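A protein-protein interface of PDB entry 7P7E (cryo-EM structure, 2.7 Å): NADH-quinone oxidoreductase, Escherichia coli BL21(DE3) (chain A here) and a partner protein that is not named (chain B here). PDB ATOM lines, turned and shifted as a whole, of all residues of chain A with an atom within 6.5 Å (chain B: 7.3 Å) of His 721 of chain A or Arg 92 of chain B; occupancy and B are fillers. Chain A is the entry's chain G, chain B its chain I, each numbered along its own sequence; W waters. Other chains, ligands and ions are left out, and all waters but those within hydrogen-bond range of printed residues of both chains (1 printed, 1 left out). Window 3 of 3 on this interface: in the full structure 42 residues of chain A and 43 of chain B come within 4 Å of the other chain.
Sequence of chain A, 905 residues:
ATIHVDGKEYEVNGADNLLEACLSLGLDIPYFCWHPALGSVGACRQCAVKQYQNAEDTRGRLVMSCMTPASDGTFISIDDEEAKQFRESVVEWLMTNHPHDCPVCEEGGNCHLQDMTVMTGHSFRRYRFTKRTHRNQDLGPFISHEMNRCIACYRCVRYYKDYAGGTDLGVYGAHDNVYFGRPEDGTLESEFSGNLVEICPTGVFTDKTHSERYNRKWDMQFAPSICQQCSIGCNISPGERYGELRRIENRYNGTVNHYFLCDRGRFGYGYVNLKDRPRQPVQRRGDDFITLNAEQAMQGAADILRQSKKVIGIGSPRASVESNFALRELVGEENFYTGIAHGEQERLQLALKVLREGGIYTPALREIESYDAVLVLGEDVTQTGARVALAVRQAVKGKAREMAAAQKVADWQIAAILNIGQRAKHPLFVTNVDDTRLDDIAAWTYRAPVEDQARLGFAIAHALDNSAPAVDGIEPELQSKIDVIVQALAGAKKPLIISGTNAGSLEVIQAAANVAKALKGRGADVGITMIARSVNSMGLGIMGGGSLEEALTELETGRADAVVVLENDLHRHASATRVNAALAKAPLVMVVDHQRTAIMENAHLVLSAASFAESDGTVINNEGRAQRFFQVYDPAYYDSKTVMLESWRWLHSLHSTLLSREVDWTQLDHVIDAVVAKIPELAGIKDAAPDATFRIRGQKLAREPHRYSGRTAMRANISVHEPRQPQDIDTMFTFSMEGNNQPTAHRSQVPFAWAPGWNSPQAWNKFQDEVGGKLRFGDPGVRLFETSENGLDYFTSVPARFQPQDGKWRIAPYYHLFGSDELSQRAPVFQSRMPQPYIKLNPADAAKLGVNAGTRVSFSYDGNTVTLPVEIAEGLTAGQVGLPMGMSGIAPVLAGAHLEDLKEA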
ATOM      1  N   ARG A 715      25.046  -5.060 -23.354  1.00  0.00           N
ATOM      2  CA  ARG A 715      25.509  -5.641 -24.605  1.00  0.00           C
ATOM      3  C   ARG A 715      25.150  -7.113 -24.721  1.00  0.00           C
ATOM      4  O   ARG A 715      25.677  -7.802 -25.601  1.00  0.00           O
ATOM      5  CB  ARG A 715      27.020  -5.458 -24.737  1.00  0.00           C
ATOM      6  CG  ARG A 715      27.447  -4.629 -25.924  1.00  0.00           C
ATOM      7  CD  ARG A 715      28.956  -4.615 -26.044  1.00  0.00           C
ATOM      8  NE  ARG A 715      29.476  -5.886 -26.534  1.00  0.00           N
ATOM      9  CZ  ARG A 715      29.733  -6.147 -27.808  1.00  0.00           C
ATOM     10  NH1 ARG A 715      29.541  -5.241 -28.751  1.00  0.00           N
ATOM     11  NH2 ARG A 715      30.194  -7.348 -28.143  1.00  0.00           N
ATOM     12  N   ALA A 716      24.260  -7.609 -23.857  1.00  0.00           N
ATOM     13  CA  ALA A 716      23.976  -9.037 -23.787  1.00  0.00           C
ATOM     14  C   ALA A 716      23.208  -9.552 -24.997  1.00  0.00           C
ATOM     15  O   ALA A 716      23.287 -10.747 -25.297  1.00  0.00           O
ATOM     16  CB  ALA A 716      23.200  -9.352 -22.508  1.00  0.00           C
ATOM     17  N   SER A 719      26.272 -10.174 -27.405  1.00  0.00           N
ATOM     18  CA  SER A 719      27.052 -11.288 -26.885  1.00  0.00           C
ATOM     19  C   SER A 719      26.869 -11.343 -25.377  1.00  0.00           C
ATOM     20  O   SER A 719      26.928 -10.309 -24.708  1.00  0.00           O
ATOM     21  CB  SER A 719      28.534 -11.143 -27.238  1.00  0.00           C
ATOM     22  OG  SER A 719      29.312 -12.132 -26.588  1.00  0.00           O
ATOM     23  N   VAL A 720      26.644 -12.550 -24.851  1.00  0.00           N
ATOM     24  CA  VAL A 720      26.501 -12.721 -23.410  1.00  0.00           C
ATOM     25  C   VAL A 720      27.826 -12.494 -22.690  1.00  0.00           C
ATOM     26  O   VAL A 720      27.833 -12.158 -21.501  1.00  0.00           O
ATOM     27  CB  VAL A 720      25.899 -14.111 -23.105  1.00  0.00           C
ATOM     28  CG1 VAL A 720      26.916 -15.224 -23.328  1.00  0.00           C
ATOM     29  CG2 VAL A 720      25.323 -14.164 -21.694  1.00  0.00           C
ATOM     30  N   HIS A 721      28.951 -12.636 -23.387  1.00  0.00           N
ATOM     31  CA  HIS A 721      30.248 -12.355 -22.793  1.00  0.00           C
ATOM     32  C   HIS A 721      30.462 -10.850 -22.725  1.00  0.00           C
ATOM     33  O   HIS A 721      30.314 -10.148 -23.730  1.00  0.00           O
ATOM     34  CB  HIS A 721      31.359 -13.016 -23.605  1.00  0.00           C
ATOM     35  CG  HIS A 721      31.201 -14.497 -23.746  1.00  0.00           C
ATOM     36  ND1 HIS A 721      31.766 -15.392 -22.863  1.00  0.00           N
ATOM     37  CD2 HIS A 721      30.532 -15.239 -24.659  1.00  0.00           C
ATOM     38  CE1 HIS A 721      31.457 -16.623 -23.231  1.00  0.00           C
ATOM     39  NE2 HIS A 721      30.708 -16.558 -24.316  1.00  0.00           N
ATOM     40  N   GLU A 722      30.790 -10.358 -21.539  1.00  0.00           N
ATOM     41  CA  GLU A 722      31.047  -8.935 -21.367  1.00  0.00           C
ATOM     42  C   GLU A 722      32.343  -8.562 -22.076  1.00  0.00           C
ATOM     43  O   GLU A 722      33.359  -9.245 -21.900  1.00  0.00           O
ATOM     44  CB  GLU A 722      31.129  -8.575 -19.887  1.00  0.00           C
ATOM     45  CG  GLU A 722      29.796  -8.627 -19.166  1.00  0.00           C
ATOM     46  CD  GLU A 722      29.485 -10.004 -18.620  1.00  0.00           C
ATOM     47  OE1 GLU A 722      30.421 -10.684 -18.151  1.00  0.00           O
ATOM     48  OE2 GLU A 722      28.306 -10.412 -18.668  1.00  0.00           O
ATOM     49  N   PRO A 723      32.353  -7.506 -22.875  1.00  0.00           N
ATOM     50  CA  PRO A 723      33.550  -7.149 -23.638  1.00  0.00           C
ATOM     51  C   PRO A 723      34.586  -6.483 -22.741  1.00  0.00           C
ATOM     52  O   PRO A 723      34.353  -6.215 -21.563  1.00  0.00           O
ATOM     53  CB  PRO A 723      33.007  -6.176 -24.682  1.00  0.00           C
ATOM     54  CG  PRO A 723      31.896  -5.492 -23.973  1.00  0.00           C
ATOM     55  CD  PRO A 723      31.265  -6.534 -23.078  1.00  0.00           C
ATOM     56  N   ASN B  60      19.981 -10.844 -18.143  1.00  0.00           N
ATOM     57  CA  ASN B  60      21.006 -11.867 -18.319  1.00  0.00           C
ATOM     58  C   ASN B  60      20.864 -12.862 -17.175  1.00  0.00           C
ATOM     59  O   ASN B  60      21.373 -12.638 -16.076  1.00  0.00           O
ATOM     60  CB  ASN B  60      22.391 -11.231 -18.348  1.00  0.00           C
ATOM     61  CG  ASN B  60      23.469 -12.185 -18.817  1.00  0.00           C
ATOM     62  OD1 ASN B  60      23.206 -13.349 -19.112  1.00  0.00           O
ATOM     63  ND2 ASN B  60      24.696 -11.693 -18.889  1.00  0.00           N
ATOM     64  N   PHE B  61      20.166 -13.967 -17.429  1.00  0.00           N
ATOM     65  CA  PHE B  61      19.921 -14.954 -16.388  1.00  0.00           C
ATOM     66  C   PHE B  61      21.132 -15.825 -16.095  1.00  0.00           C
ATOM     67  O   PHE B  61      21.135 -16.526 -15.080  1.00  0.00           O
ATOM     68  CB  PHE B  61      18.730 -15.834 -16.762  1.00  0.00           C
ATOM     69  CG  PHE B  61      17.410 -15.245 -16.377  1.00  0.00           C
ATOM     70  CD1 PHE B  61      17.100 -15.017 -15.049  1.00  0.00           C
ATOM     71  CD2 PHE B  61      16.485 -14.902 -17.343  1.00  0.00           C
ATOM     72  CE1 PHE B  61      15.888 -14.468 -14.695  1.00  0.00           C
ATOM     73  CE2 PHE B  61      15.271 -14.355 -16.995  1.00  0.00           C
ATOM     74  CZ  PHE B  61      14.973 -14.139 -15.673  1.00  0.00           C
ATOM     75  N   SER B  62      22.157 -15.797 -16.948  1.00  0.00           N
ATOM     76  CA  SER B  62      23.418 -16.433 -16.597  1.00  0.00           C
ATOM     77  C   SER B  62      24.148 -15.670 -15.503  1.00  0.00           C
ATOM     78  O   SER B  62      25.016 -16.242 -14.838  1.00  0.00           O
ATOM     79  CB  SER B  62      24.308 -16.563 -17.834  1.00  0.00           C
ATOM     80  OG  SER B  62      24.965 -15.345 -18.127  1.00  0.00           O
ATOM     81  N   ARG B  63      23.812 -14.397 -15.301  1.00  0.00           N
ATOM     82  CA  ARG B  63      24.397 -13.581 -14.250  1.00  0.00           C
ATOM     83  C   ARG B  63      23.501 -13.436 -13.029  1.00  0.00           C
ATOM     84  O   ARG B  63      24.014 -13.161 -11.940  1.00  0.00           O
ATOM     85  CB  ARG B  63      24.720 -12.180 -14.783  1.00  0.00           C
ATOM     86  CG  ARG B  63      25.992 -12.095 -15.588  1.00  0.00           C
ATOM     87  CD  ARG B  63      27.163 -11.736 -14.702  1.00  0.00           C
ATOM     88  NE  ARG B  63      28.368 -11.474 -15.476  1.00  0.00           N
ATOM     89  CZ  ARG B  63      29.581 -11.365 -14.955  1.00  0.00           C
ATOM     90  NH1 ARG B  63      29.788 -11.495 -13.656  1.00  0.00           N
ATOM     91  NH2 ARG B  63      30.611 -11.120 -15.757  1.00  0.00           N
ATOM     92  N   GLU B  89      19.626 -24.317 -19.951  1.00  0.00           N
ATOM     93  CA  GLU B  89      19.771 -24.046 -21.373  1.00  0.00           C
ATOM     94  C   GLU B  89      20.985 -24.782 -21.917  1.00  0.00           C
ATOM     95  O   GLU B  89      21.788 -25.346 -21.171  1.00  0.00           O
ATOM     96  CB  GLU B  89      19.911 -22.544 -21.654  1.00  0.00           C
ATOM     97  CG  GLU B  89      18.612 -21.760 -21.603  1.00  0.00           C
ATOM     98  CD  GLU B  89      17.737 -21.974 -22.824  1.00  0.00           C
ATOM     99  OE1 GLU B  89      18.221 -22.542 -23.824  1.00  0.00           O
ATOM    100  OE2 GLU B  89      16.559 -21.563 -22.782  1.00  0.00           O
ATOM    101  N   TYR B  90      21.112 -24.767 -23.243  1.00  0.00           N
ATOM    102  CA  TYR B  90      22.266 -25.343 -23.921  1.00  0.00           C
ATOM    103  C   TYR B  90      23.346 -24.307 -24.200  1.00  0.00           C
ATOM    104  O   TYR B  90      24.536 -24.596 -24.041  1.00  0.00           O
ATOM    105  CB  TYR B  90      21.837 -26.002 -25.234  1.00  0.00           C
ATOM    106  CG  TYR B  90      20.944 -27.205 -25.057  1.00  0.00           C
ATOM    107  CD1 TYR B  90      21.463 -28.422 -24.640  1.00  0.00           C
ATOM    108  CD2 TYR B  90      19.582 -27.126 -25.311  1.00  0.00           C
ATOM    109  CE1 TYR B  90      20.652 -29.527 -24.479  1.00  0.00           C
ATOM    110  CE2 TYR B  90      18.763 -28.224 -25.151  1.00  0.00           C
ATOM    111  CZ  TYR B  90      19.303 -29.420 -24.736  1.00  0.00           C
ATOM    112  OH  TYR B  90      18.492 -30.518 -24.576  1.00  0.00           O
ATOM    113  N   LYS B  91      22.956 -23.108 -24.615  1.00  0.00           N
ATOM    114  CA  LYS B  91      23.888 -22.028 -24.895  1.00  0.00           C
ATOM    115  C   LYS B  91      23.666 -20.882 -23.919  1.00  0.00           C
ATOM    116  O   LYS B  91      22.542 -20.629 -23.479  1.00  0.00           O
ATOM    117  CB  LYS B  91      23.735 -21.527 -26.331  1.00  0.00           C
ATOM    118  CG  LYS B  91      23.434 -22.619 -27.336  1.00  0.00           C
ATOM    119  CD  LYS B  91      24.701 -23.339 -27.760  1.00  0.00           C
ATOM    120  CE  LYS B  91      25.672 -22.395 -28.444  1.00  0.00           C
ATOM    121  NZ  LYS B  91      26.625 -23.124 -29.325  1.00  0.00           N
ATOM    122  N   ARG B  92      24.757 -20.192 -23.579  1.00  0.00           N
ATOM    123  CA  ARG B  92      24.673 -19.093 -22.624  1.00  0.00           C
ATOM    124  C   ARG B  92      23.961 -17.882 -23.208  1.00  0.00           C
ATOM    125  O   ARG B  92      23.366 -17.100 -22.459  1.00  0.00           O
ATOM    126  CB  ARG B  92      26.068 -18.698 -22.151  1.00  0.00           C
ATOM    127  CG  ARG B  92      26.213 -18.676 -20.653  1.00  0.00           C
ATOM    128  CD  ARG B  92      27.590 -18.208 -20.260  1.00  0.00           C
ATOM    129  NE  ARG B  92      27.619 -16.774 -20.009  1.00  0.00           N
ATOM    130  CZ  ARG B  92      28.725 -16.048 -19.951  1.00  0.00           C
ATOM    131  NH1 ARG B  92      29.918 -16.592 -20.123  1.00  0.00           N
ATOM    132  NH2 ARG B  92      28.632 -14.744 -19.713  1.00  0.00           N
ATOM    133  N   GLN B  93      24.017 -17.706 -24.530  1.00  0.00           N
ATOM    134  CA  GLN B  93      23.281 -16.623 -25.176  1.00  0.00           C
ATOM    135  C   GLN B  93      21.777 -16.802 -25.024  1.00  0.00           C
ATOM    136  O   GLN B  93      21.032 -15.817 -25.008  1.00  0.00           O
ATOM    137  CB  GLN B  93      23.662 -16.546 -26.655  1.00  0.00           C
ATOM    138  CG  GLN B  93      23.199 -15.287 -27.363  1.00  0.00           C
ATOM    139  CD  GLN B  93      23.855 -14.042 -26.816  1.00  0.00           C
ATOM    140  OE1 GLN B  93      25.079 -13.954 -26.753  1.00  0.00           O
ATOM    141  NE2 GLN B  93      23.046 -13.071 -26.416  1.00  0.00           N
ATOM    142  N   ASP B  94      21.318 -18.042 -24.891  1.00  0.00           N
ATOM    143  CA  ASP B  94      19.904 -18.333 -24.726  1.00  0.00           C
ATOM    144  C   ASP B  94      19.391 -18.017 -23.327  1.00  0.00           C
ATOM    145  O   ASP B  94      18.176 -18.036 -23.114  1.00  0.00           O
ATOM    146  CB  ASP B  94      19.650 -19.799 -25.061  1.00  0.00           C
ATOM    147  CG  ASP B  94      19.763 -20.075 -26.539  1.00  0.00           C
ATOM    148  OD1 ASP B  94      19.506 -19.150 -27.336  1.00  0.00           O
ATOM    149  OD2 ASP B  94      20.116 -21.214 -26.909  1.00  0.00           O
ATOM    150  N   LEU B  95      20.279 -17.730 -22.379  1.00  0.00           N
ATOM    151  CA  LEU B  95      19.880 -17.277 -21.054  1.00  0.00           C
ATOM    152  C   LEU B  95      19.642 -15.775 -20.994  1.00  0.00           C
ATOM    153  O   LEU B  95      19.298 -15.263 -19.924  1.00  0.00           O
ATOM    154  CB  LEU B  95      20.934 -17.678 -20.020  1.00  0.00           C
ATOM    155  CG  LEU B  95      20.905 -19.144 -19.591  1.00  0.00           C
ATOM    156  CD1 LEU B  95      22.108 -19.483 -18.736  1.00  0.00           C
ATOM    157  CD2 LEU B  95      19.618 -19.445 -18.847  1.00  0.00           C
ATOM    158  N   VAL B  96      19.825 -15.058 -22.096  1.00  0.00           N
ATOM    159  CA  VAL B  96      19.463 -13.649 -22.177  1.00  0.00           C
ATOM    160  C   VAL B  96      17.995 -13.580 -22.577  1.00  0.00           C
ATOM    161  O   VAL B  96      17.642 -13.821 -23.734  1.00  0.00           O
ATOM    162  CB  VAL B  96      20.353 -12.892 -23.169  1.00  0.00           C
ATOM    163  CG1 VAL B  96      19.953 -11.430 -23.225  1.00  0.00           C
ATOM    164  CG2 VAL B  96      21.812 -13.029 -22.778  1.00  0.00           C
HETATM  165  O   HOH W   1      30.534 -13.651 -18.694  1.00  0.00           O
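Water W1 bridges NH2 of Arg 92 of chain B (2.4 Å) and OE1 of Glu 722 of chain A (3.0 Å).
OE1 of Glu 722 of chain A is in salt-bridge range of NH2 of Arg 63 of chain B (2.4 Å). The backbone carbonyl oxygen of Ala 716 of chain A is in hydrogen-bond range of the side-chain amide nitrogen of Gln 93 of chain B (2.6 Å). The guanidinium group of Arg 92 of chain B is in hydrogen-bond range of the backbone carbonyl oxygen of Val 720 of chain A, at 3.2 Å. The backbone NH of Val 720 of chain A sits at hydrogen-bond distance from the side-chain amide oxygen of Gln 93 of chain B.
OD1 of Asn 60 of chain B lies within hydrogen-bond range of OG of Ser 62 of chain B, at 2.8 Å. The side-chain hydroxyl (OG) of Ser 719 of chain A lies close to the backbone NH (N) of His 721 of chain A.
Of the 12 printed residues of chain B, 6 touch a printed residue of chain A. Printed residues of chain B that touch a printed residue of chain A: Asn 60, Ser 62, Arg 63, Arg 92, Gln 93 and Val 96. Hydrophobic or aromatic side chains of chain B within 4 Å of the printed part of chain A: Val 96. Hydrophobic or aromatic side chains of chain A that line the printed part of chain B: Ala 716, Val 720 and His 721. Among the printed residues, 11 pairs touch across the chains. Among the printed residues, Asp or Glu carboxylates within 4 Å of a Lys or Arg side-chain nitrogen of the other chain: Glu 722 of chain A with Arg 63 of chain B (2.4 Å).
Among the printed residues, pairs that only touch across the chains: Ser 719 of chain A with Gln 93 of chain B (3.3 Å), Val 720 of chain A with Asn 60 of chain B (3.4 Å), His 721 of chain A with Arg 92 of chain B (3.5 Å), Ala 716 of chain A with Val 96 of chain B (3.7 Å), Val 720 of chain A with Ser 62 of chain B (3.8 Å), Glu 722 of chain A with Asn 60 of chain B (3.8 Å) and Val 720 of chain A with Val 96 of chain B (3.8 Å).
His 721 of chain A touches one residue of chain B. Printed residues of chain B within 4 Å of Glu 722 of chain A: Asn 60 and Arg 63. Of the printed residues of chain A, Asn 60 of chain B touches Val 720 and Glu 722. Printed residues of chain A within 4 Å of Ser 62 of chain B: Val 720. Tyr 90 of chain B touches none of the printed residues of chain A. Of chain A, only Val 720 and His 721 come within 4 Å of Arg 92 of chain B. The nearest residue of chain A that does not touch Arg 92 of chain B is Glu 722 of chain A (4.5 Å). The nearest printed residue of chain A that does not touch Asn 60 of chain B is Ala 716 of chain A (4.6 Å).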
